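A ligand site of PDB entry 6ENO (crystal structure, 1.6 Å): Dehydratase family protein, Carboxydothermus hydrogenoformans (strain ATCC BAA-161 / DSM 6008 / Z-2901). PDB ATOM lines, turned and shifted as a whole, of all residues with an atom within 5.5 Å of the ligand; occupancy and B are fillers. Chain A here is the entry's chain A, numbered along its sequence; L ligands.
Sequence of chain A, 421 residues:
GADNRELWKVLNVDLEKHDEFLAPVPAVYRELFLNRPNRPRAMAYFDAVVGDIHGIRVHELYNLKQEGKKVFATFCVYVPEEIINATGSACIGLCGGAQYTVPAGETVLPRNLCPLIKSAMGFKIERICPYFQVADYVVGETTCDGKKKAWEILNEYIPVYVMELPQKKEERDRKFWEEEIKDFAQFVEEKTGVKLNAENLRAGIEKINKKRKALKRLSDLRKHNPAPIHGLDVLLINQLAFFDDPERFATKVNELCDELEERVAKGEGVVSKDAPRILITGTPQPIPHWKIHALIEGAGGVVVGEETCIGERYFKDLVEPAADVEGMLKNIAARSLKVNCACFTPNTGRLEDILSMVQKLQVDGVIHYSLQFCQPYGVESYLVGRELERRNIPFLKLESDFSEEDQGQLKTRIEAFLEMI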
ATOM      1  N   PHE A  75     -23.563  23.765  -0.447  1.00  0.00           N
ATOM      2  CA  PHE A  75     -23.112  22.379  -0.278  1.00  0.00           C
ATOM      3  C   PHE A  75     -23.643  21.458  -1.364  1.00  0.00           C
ATOM      4  O   PHE A  75     -23.427  20.226  -1.265  1.00  0.00           O
ATOM      5  CB  PHE A  75     -23.537  21.845   1.095  1.00  0.00           C
ATOM      6  CG  PHE A  75     -22.890  22.576   2.207  1.00  0.00           C
ATOM      7  CD1 PHE A  75     -23.426  23.771   2.668  1.00  0.00           C
ATOM      8  CD2 PHE A  75     -21.731  22.114   2.773  1.00  0.00           C
ATOM      9  CE1 PHE A  75     -22.828  24.475   3.678  1.00  0.00           C
ATOM     10  CE2 PHE A  75     -21.109  22.839   3.785  1.00  0.00           C
ATOM     11  CZ  PHE A  75     -21.671  23.993   4.235  1.00  0.00           C
ATOM     12  N   CYS A  76     -24.270  21.992  -2.396  1.00  0.00           N
ATOM     13  CA  CYS A  76     -24.838  21.171  -3.453  1.00  0.00           C
ATOM     14  C   CYS A  76     -24.816  21.908  -4.775  1.00  0.00           C
ATOM     15  O   CYS A  76     -25.075  23.117  -4.822  1.00  0.00           O
ATOM     16  CB  CYS A  76     -26.283  20.812  -3.114  1.00  0.00           C
ATOM     17  SG  CYS A  76     -27.179  19.795  -4.291  1.00  0.00           S
ATOM     18  N   VAL A  77     -24.557  21.169  -5.859  1.00  0.00           N
ATOM     19  CA  VAL A  77     -24.542  21.736  -7.206  1.00  0.00           C
ATOM     20  C   VAL A  77     -25.890  22.262  -7.658  1.00  0.00           C
ATOM     21  O   VAL A  77     -25.950  23.038  -8.623  1.00  0.00           O
ATOM     22  CB  VAL A  77     -24.021  20.707  -8.238  1.00  0.00           C
ATOM     23  CG1 VAL A  77     -22.638  20.187  -7.796  1.00  0.00           C
ATOM     24  CG2 VAL A  77     -25.016  19.516  -8.510  1.00  0.00           C
ATOM     25  N   TYR A  78     -26.986  21.885  -6.996  1.00  0.00           N
ATOM     26  CA  TYR A  78     -28.304  22.361  -7.379  1.00  0.00           C
ATOM     27  C   TYR A  78     -28.529  23.825  -7.026  1.00  0.00           C
ATOM     28  O   TYR A  78     -29.418  24.463  -7.614  1.00  0.00           O
ATOM     29  CB  TYR A  78     -29.391  21.502  -6.706  1.00  0.00           C
ATOM     30  CG  TYR A  78     -29.899  20.374  -7.574  1.00  0.00           C
ATOM     31  CD1 TYR A  78     -29.203  19.200  -7.683  1.00  0.00           C
ATOM     32  CD2 TYR A  78     -31.062  20.516  -8.337  1.00  0.00           C
ATOM     33  CE1 TYR A  78     -29.628  18.179  -8.516  1.00  0.00           C
ATOM     34  CE2 TYR A  78     -31.504  19.490  -9.155  1.00  0.00           C
ATOM     35  CZ  TYR A  78     -30.772  18.319  -9.227  1.00  0.00           C
ATOM     36  OH  TYR A  78     -31.184  17.303 -10.063  1.00  0.00           O
ATOM     37  N   CYS A  95     -18.462  21.843   1.065  1.00  0.00           N
ATOM     38  CA  CYS A  95     -18.528  20.435   1.438  1.00  0.00           C
ATOM     39  C   CYS A  95     -17.219  20.019   2.113  1.00  0.00           C
ATOM     40  O   CYS A  95     -16.128  20.320   1.605  1.00  0.00           O
ATOM     41  CB  CYS A  95     -18.792  19.568   0.210  1.00  0.00           C
ATOM     42  SG  CYS A  95     -20.471  19.679  -0.448  1.00  0.00           S
ATOM     43  N   CYS A 114     -22.693  10.736   7.295  1.00  0.00           N
ATOM     44  CA  CYS A 114     -21.704  11.016   6.259  1.00  0.00           C
ATOM     45  C   CYS A 114     -20.596  11.902   6.807  1.00  0.00           C
ATOM     46  O   CYS A 114     -20.877  12.922   7.451  1.00  0.00           O
ATOM     47  CB  CYS A 114     -22.353  11.694   5.059  1.00  0.00           C
ATOM     48  SG  CYS A 114     -21.229  11.999   3.667  1.00  0.00           S
ATOM     49  N   LEU A 116     -18.677  13.898   5.118  1.00  0.00           N
ATOM     50  CA  LEU A 116     -18.753  15.214   4.479  1.00  0.00           C
ATOM     51  C   LEU A 116     -19.531  16.179   5.362  1.00  0.00           C
ATOM     52  O   LEU A 116     -19.121  17.332   5.570  1.00  0.00           O
ATOM     53  CB  LEU A 116     -19.408  15.068   3.112  1.00  0.00           C
ATOM     54  CG  LEU A 116     -19.491  16.278   2.210  1.00  0.00           C
ATOM     55  CD1 LEU A 116     -19.680  15.784   0.778  1.00  0.00           C
ATOM     56  CD2 LEU A 116     -20.694  17.146   2.610  1.00  0.00           C
ATOM     57  N   ILE A 117     -20.659  15.712   5.894  1.00  0.00           N
ATOM     58  CA  ILE A 117     -21.516  16.546   6.727  1.00  0.00           C
ATOM     59  C   ILE A 117     -20.857  16.820   8.064  1.00  0.00           C
ATOM     60  O   ILE A 117     -20.818  17.948   8.550  1.00  0.00           O
ATOM     61  CB  ILE A 117     -22.902  15.881   6.901  1.00  0.00           C
ATOM     62  CG1 ILE A 117     -23.465  15.484   5.526  1.00  0.00           C
ATOM     63  CG2 ILE A 117     -23.867  16.804   7.654  1.00  0.00           C
ATOM     64  CD1 ILE A 117     -24.693  14.566   5.678  1.00  0.00           C
ATOM     65  N   GLU A 141     -29.959  22.515   1.252  1.00  0.00           N
ATOM     66  CA  GLU A 141     -30.907  21.900   0.322  1.00  0.00           C
ATOM     67  C   GLU A 141     -31.424  20.582   0.918  1.00  0.00           C
ATOM     68  O   GLU A 141     -30.721  19.949   1.695  1.00  0.00           O
ATOM     69  CB  GLU A 141     -30.201  21.694  -1.035  1.00  0.00           C
ATOM     70  CG  GLU A 141     -29.392  20.419  -1.212  1.00  0.00           C
ATOM     71  CD  GLU A 141     -28.065  20.306  -0.448  1.00  0.00           C
ATOM     72  OE1 GLU A 141     -27.620  21.264   0.216  1.00  0.00           O
ATOM     73  OE2 GLU A 141     -27.416  19.232  -0.547  1.00  0.00           O
ATOM     74  N   THR A 143     -31.659  17.357   0.160  1.00  0.00           N
ATOM     75  CA  THR A 143     -31.191  16.177  -0.552  1.00  0.00           C
ATOM     76  C   THR A 143     -31.188  14.972   0.382  1.00  0.00           C
ATOM     77  O   THR A 143     -32.263  14.384   0.574  1.00  0.00           O
ATOM     78  CB  THR A 143     -29.815  16.403  -1.133  1.00  0.00           C
ATOM     79  OG1 THR A 143     -29.030  17.027  -0.127  1.00  0.00           O
ATOM     80  CG2 THR A 143     -29.874  17.299  -2.357  1.00  0.00           C
ATOM     81  N   CYS A 144     -30.047  14.623   0.976  1.00  0.00           N
ATOM     82  CA  CYS A 144     -29.989  13.430   1.825  1.00  0.00           C
ATOM     83  C   CYS A 144     -30.496  13.743   3.221  1.00  0.00           C
ATOM     84  O   CYS A 144     -30.597  14.899   3.621  1.00  0.00           O
ATOM     85  CB  CYS A 144     -28.580  12.889   1.929  1.00  0.00           C
ATOM     86  SG  CYS A 144     -27.425  14.095   2.622  1.00  0.00           S
ATOM     87  N   LYS A 147     -28.002  15.786   5.569  1.00  0.00           N
ATOM     88  CA  LYS A 147     -27.883  17.221   5.285  1.00  0.00           C
ATOM     89  C   LYS A 147     -29.139  17.939   5.734  1.00  0.00           C
ATOM     90  O   LYS A 147     -29.074  18.963   6.407  1.00  0.00           O
ATOM     91  CB  LYS A 147     -27.644  17.488   3.810  1.00  0.00           C
ATOM     92  CG  LYS A 147     -26.179  17.409   3.383  1.00  0.00           C
ATOM     93  CD  LYS A 147     -26.099  17.354   1.851  1.00  0.00           C
ATOM     94  CE  LYS A 147     -24.899  18.093   1.311  1.00  0.00           C
ATOM     95  NZ  LYS A 147     -24.966  18.187  -0.162  1.00  0.00           N
ATOM     96  N   THR A 283     -20.037   9.424  -4.948  1.00  0.00           N
ATOM     97  CA  THR A 283     -20.205  10.660  -4.200  1.00  0.00           C
ATOM     98  C   THR A 283     -19.058  11.629  -4.485  1.00  0.00           C
ATOM     99  O   THR A 283     -17.965  11.225  -4.904  1.00  0.00           O
ATOM    100  CB  THR A 283     -20.270  10.372  -2.693  1.00  0.00           C
ATOM    101  OG1 THR A 283     -19.224   9.457  -2.338  1.00  0.00           O
ATOM    102  CG2 THR A 283     -21.613   9.712  -2.285  1.00  0.00           C
ATOM    103  N   PRO A 284     -19.277  12.926  -4.242  1.00  0.00           N
ATOM    104  CA  PRO A 284     -18.184  13.896  -4.448  1.00  0.00           C
ATOM    105  C   PRO A 284     -17.079  13.662  -3.440  1.00  0.00           C
ATOM    106  O   PRO A 284     -17.301  13.160  -2.338  1.00  0.00           O
ATOM    107  CB  PRO A 284     -18.860  15.246  -4.234  1.00  0.00           C
ATOM    108  CG  PRO A 284     -20.141  14.959  -3.471  1.00  0.00           C
ATOM    109  CD  PRO A 284     -20.528  13.559  -3.803  1.00  0.00           C
ATOM    110  N   CYS A 309     -20.317  14.813  -8.414  1.00  0.00           N
ATOM    111  CA  CYS A 309     -20.500  16.258  -8.393  1.00  0.00           C
ATOM    112  C   CYS A 309     -19.235  17.055  -8.100  1.00  0.00           C
ATOM    113  O   CYS A 309     -19.320  18.279  -8.121  1.00  0.00           O
ATOM    114  CB  CYS A 309     -21.571  16.630  -7.372  1.00  0.00           C
ATOM    115  SG  CYS A 309     -23.240  16.343  -7.977  1.00  0.00           S
ATOM    116  N   ARG A 313     -20.750  15.587 -12.889  1.00  0.00           N
ATOM    117  CA  ARG A 313     -22.106  16.092 -12.629  1.00  0.00           C
ATOM    118  C   ARG A 313     -22.107  17.587 -12.367  1.00  0.00           C
ATOM    119  O   ARG A 313     -23.166  18.220 -12.505  1.00  0.00           O
ATOM    120  CB  ARG A 313     -22.779  15.378 -11.445  1.00  0.00           C
ATOM    121  CG  ARG A 313     -22.989  13.860 -11.666  1.00  0.00           C
ATOM    122  CD  ARG A 313     -23.974  13.245 -10.658  1.00  0.00           C
ATOM    123  NE  ARG A 313     -23.499  13.345  -9.284  1.00  0.00           N
ATOM    124  CZ  ARG A 313     -22.928  12.368  -8.585  1.00  0.00           C
ATOM    125  NH1 ARG A 313     -22.763  11.149  -9.122  1.00  0.00           N
ATOM    126  NH2 ARG A 313     -22.561  12.596  -7.342  1.00  0.00           N
ATOM    127  N   VAL A 339     -29.132  17.322 -13.300  1.00  0.00           N
ATOM    128  CA  VAL A 339     -28.152  16.567 -12.533  1.00  0.00           C
ATOM    129  C   VAL A 339     -28.793  15.284 -12.003  1.00  0.00           C
ATOM    130  O   VAL A 339     -29.800  15.313 -11.299  1.00  0.00           O
ATOM    131  CB  VAL A 339     -27.581  17.438 -11.405  1.00  0.00           C
ATOM    132  CG1 VAL A 339     -26.664  16.603 -10.514  1.00  0.00           C
ATOM    133  CG2 VAL A 339     -26.811  18.620 -11.998  1.00  0.00           C
ATOM    134  N   CYS A 341     -28.574  12.995  -9.609  1.00  0.00           N
ATOM    135  CA  CYS A 341     -28.167  12.612  -8.266  1.00  0.00           C
ATOM    136  C   CYS A 341     -29.040  11.467  -7.746  1.00  0.00           C
ATOM    137  O   CYS A 341     -30.237  11.403  -8.034  1.00  0.00           O
ATOM    138  CB  CYS A 341     -28.296  13.827  -7.354  1.00  0.00           C
ATOM    139  SG  CYS A 341     -28.027  13.479  -5.600  1.00  0.00           S
ATOM    140  N   ALA A 342     -28.440  10.584  -6.928  1.00  0.00           N
ATOM    141  CA  ALA A 342     -29.153   9.437  -6.373  1.00  0.00           C
ATOM    142  C   ALA A 342     -30.256   9.806  -5.402  1.00  0.00           C
ATOM    143  O   ALA A 342     -31.018   8.905  -5.012  1.00  0.00           O
ATOM    144  CB  ALA A 342     -28.194   8.459  -5.677  1.00  0.00           C
ATOM    145  N   CYS A 343     -30.378  11.084  -5.004  1.00  0.00           N
ATOM    146  CA  CYS A 343     -31.520  11.498  -4.196  1.00  0.00           C
ATOM    147  C   CYS A 343     -32.806  11.543  -4.986  1.00  0.00           C
ATOM    148  O   CYS A 343     -33.883  11.709  -4.399  1.00  0.00           O
ATOM    149  CB  CYS A 343     -31.240  12.886  -3.572  1.00  0.00           C
ATOM    150  SG  CYS A 343     -29.792  12.812  -2.432  1.00  0.00           S
ATOM    151  N   LEU A 371     -19.055   7.554   0.092  1.00  0.00           N
ATOM    152  CA  LEU A 371     -18.726   7.800   1.488  1.00  0.00           C
ATOM    153  C   LEU A 371     -19.591   6.927   2.415  1.00  0.00           C
ATOM    154  O   LEU A 371     -20.759   6.634   2.142  1.00  0.00           O
ATOM    155  CB  LEU A 371     -18.930   9.283   1.820  1.00  0.00           C
ATOM    156  CG  LEU A 371     -18.104  10.294   1.014  1.00  0.00           C
ATOM    157  CD1 LEU A 371     -18.425  11.703   1.480  1.00  0.00           C
ATOM    158  CD2 LEU A 371     -16.613  10.003   1.166  1.00  0.00           C
ATOM    159  N   PHE A 373     -22.007   5.736   5.097  1.00  0.00           N
ATOM    160  CA  PHE A 373     -23.287   6.214   5.587  1.00  0.00           C
ATOM    161  C   PHE A 373     -23.991   7.117   4.581  1.00  0.00           C
ATOM    162  O   PHE A 373     -25.011   7.722   4.945  1.00  0.00           O
ATOM    163  CB  PHE A 373     -23.127   6.961   6.921  1.00  0.00           C
ATOM    164  CG  PHE A 373     -22.383   6.173   7.947  1.00  0.00           C
ATOM    165  CD1 PHE A 373     -22.738   4.874   8.234  1.00  0.00           C
ATOM    166  CD2 PHE A 373     -21.306   6.731   8.613  1.00  0.00           C
ATOM    167  CE1 PHE A 373     -22.052   4.145   9.181  1.00  0.00           C
ATOM    168  CE2 PHE A 373     -20.602   6.015   9.560  1.00  0.00           C
ATOM    169  CZ  PHE A 373     -20.973   4.716   9.840  1.00  0.00           C
ATOM    170  N   CYS A 374     -23.517   7.231   3.343  1.00  0.00           N
ATOM    171  CA  CYS A 374     -24.275   7.913   2.292  1.00  0.00           C
ATOM    172  C   CYS A 374     -25.242   6.879   1.735  1.00  0.00           C
ATOM    173  O   CYS A 374     -24.857   6.019   0.933  1.00  0.00           O
ATOM    174  CB  CYS A 374     -23.397   8.466   1.175  1.00  0.00           C
ATOM    175  SG  CYS A 374     -24.411   9.055  -0.229  1.00  0.00           S
ATOM    176  N   GLN A 375     -26.482   6.978   2.147  1.00  0.00           N
ATOM    177  CA  GLN A 375     -27.449   5.919   1.860  1.00  0.00           C
ATOM    178  C   GLN A 375     -28.001   6.047   0.453  1.00  0.00           C
ATOM    179  O   GLN A 375     -28.181   5.007  -0.209  1.00  0.00           O
ATOM    180  CB  GLN A 375     -28.540   5.920   2.947  1.00  0.00           C
ATOM    181  CG  GLN A 375     -27.925   5.607   4.309  1.00  0.00           C
ATOM    182  CD  GLN A 375     -28.848   5.519   5.513  1.00  0.00           C
ATOM    183  OE1 GLN A 375     -28.638   4.681   6.403  1.00  0.00           O
ATOM    184  NE2 GLN A 375     -29.837   6.400   5.593  1.00  0.00           N
ATOM    185  N   PRO A 376     -28.226   7.249  -0.094  1.00  0.00           N
ATOM    186  CA  PRO A 376     -28.695   7.297  -1.490  1.00  0.00           C
ATOM    187  C   PRO A 376     -27.762   6.555  -2.435  1.00  0.00           C
ATOM    188  O   PRO A 376     -28.206   5.704  -3.222  1.00  0.00           O
ATOM    189  CB  PRO A 376     -28.792   8.801  -1.789  1.00  0.00           C
ATOM    190  CG  PRO A 376     -29.159   9.396  -0.420  1.00  0.00           C
ATOM    191  CD  PRO A 376     -28.254   8.579   0.520  1.00  0.00           C
ATOM    192  N   TYR A 377     -26.461   6.888  -2.391  1.00  0.00           N
ATOM    193  CA  TYR A 377     -25.492   6.243  -3.287  1.00  0.00           C
ATOM    194  C   TYR A 377     -25.180   4.803  -2.870  1.00  0.00           C
ATOM    195  O   TYR A 377     -24.998   3.943  -3.739  1.00  0.00           O
ATOM    196  CB  TYR A 377     -24.208   7.083  -3.370  1.00  0.00           C
ATOM    197  CG  TYR A 377     -24.464   8.315  -4.221  1.00  0.00           C
ATOM    198  CD1 TYR A 377     -24.328   8.269  -5.604  1.00  0.00           C
ATOM    199  CD2 TYR A 377     -24.969   9.475  -3.659  1.00  0.00           C
ATOM    200  CE1 TYR A 377     -24.622   9.363  -6.392  1.00  0.00           C
ATOM    201  CE2 TYR A 377     -25.287  10.572  -4.448  1.00  0.00           C
ATOM    202  CZ  TYR A 377     -25.101  10.510  -5.799  1.00  0.00           C
ATOM    203  OH  TYR A 377     -25.429  11.575  -6.579  1.00  0.00           O
HETATM  204  S1  LIG L   1     -24.669  11.361   2.356  1.00  0.00           S
HETATM  205  S2  LIG L   1     -25.632  12.927  -0.649  1.00  0.00           S
HETATM  206  S3  LIG L   1     -23.663  14.703   1.887  1.00  0.00           S
HETATM  207  S4  LIG L   1     -22.164  12.205   0.067  1.00  0.00           S
HETATM  208  S5  LIG L   1     -23.810  17.873  -4.501  1.00  0.00           S
HETATM  209  S6  LIG L   1     -24.306  14.226  -4.846  1.00  0.00           S
HETATM  210  S7  LIG L   1     -26.622  16.108  -2.885  1.00  0.00           S
HETATM  211  S8  LIG L   1     -26.664  16.724  -6.404  1.00  0.00           S
HETATM  212  S9  LIG L   1     -23.054  15.693  -1.530  1.00  0.00           S
HETATM  213 FE1  LIG L   1     -23.565  13.929  -0.206  1.00  0.00          FE
HETATM  214 FE2  LIG L   1     -22.861  12.663   2.079  1.00  0.00          FE
HETATM  215 FE3  LIG L   1     -24.233  11.329   0.232  1.00  0.00          FE
HETATM  216 FE4  LIG L   1     -25.429  13.305   1.663  1.00  0.00          FE
HETATM  217 FE5  LIG L   1     -26.460  15.027  -4.802  1.00  0.00          FE
HETATM  218 FE6  LIG L   1     -26.094  17.710  -4.450  1.00  0.00          FE
HETATM  219 FE7  LIG L   1     -24.428  16.269  -5.995  1.00  0.00          FE
HETATM  220 FE8  LIG L   1     -24.381  15.886  -3.292  1.00  0.00          FE
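The side-chain amino group (NZ) of Lys 147 lies within salt-bridge range of the side-chain carboxylate (OE2) of Glu 141, at 2.7 Å.
The backbone carbonyl oxygen (O) of Val 339 is in hydrogen-bond range of the side-chain hydroxyl (OH) of Tyr 78 (2.7 Å).
The side-chain sulfur (SG) of Cys 341 sits close to the backbone NH (N) of Cys 343.
SG of Cys 144 lies close to N of Lys 147, 3.4 Å away.
OG1 of Thr 143 lies within hydrogen-bond range of OE2 of Glu 141 (2.8 Å).
The side-chain carboxylate (OE2) of Glu 141 sits close to the side-chain sulfur (SG) of Cys 76, at 3.8 Å.
OG1 of Thr 283 sits at hydrogen-bond distance from N of Leu 371, 3.1 Å away.
O of Phe 75 sits at hydrogen-bond distance from NZ of Lys 147 (2.8 Å).
An iron atom (FE5) of the ligand is bound by the side-chain sulfur (SG) of Cys 341 (2.3 Å).
The side-chain sulfur (SG) of Cys 114 binds an iron atom (FE2) of the ligand (2.4 Å).
The side-chain amino group (NZ) of Lys 147 lies close to a sulfur (S9) of the ligand (3.4 Å).
The guanidinium group (NH2) of Arg 313 lies close to a sulfur (S6) of the ligand, 3.5 Å away.
The backbone NH of Val 77 lies close to a sulfur (S5) of the ligand, 3.6 Å away.
The side-chain sulfur (SG) of Cys 76 is bound to an iron atom (FE6) of the ligand, 2.4 Å away.
S6 of the ligand sits close to OH of Tyr 377 (3.4 Å).
SG of Cys 309 binds FE7 of the ligand.
The side-chain sulfur (SG) of Cys 144 is bound to an iron atom (FE4) of the ligand, 2.4 Å away.
SG of Cys 374 is bound to FE3 of the ligand (2.3 Å).
The side-chain hydroxyl (OG1) of Thr 143 lies close to a sulfur (S7) of the ligand (3.8 Å).
Residues that only touch the ligand: Thr 283, Pro 284, Ile 117, Tyr 78, Leu 116 and Glu 141.
Hydrophobic or aromatic side chains that line the ligand: Val 77, Tyr 78, Leu 116, Ile 117, Pro 284 and Tyr 377.
Of the 26 residues printed, 17 come within 4 Å of the ligand.
The nearest printed residue that does not touch the ligand is Phe 75 (4.02 Å).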
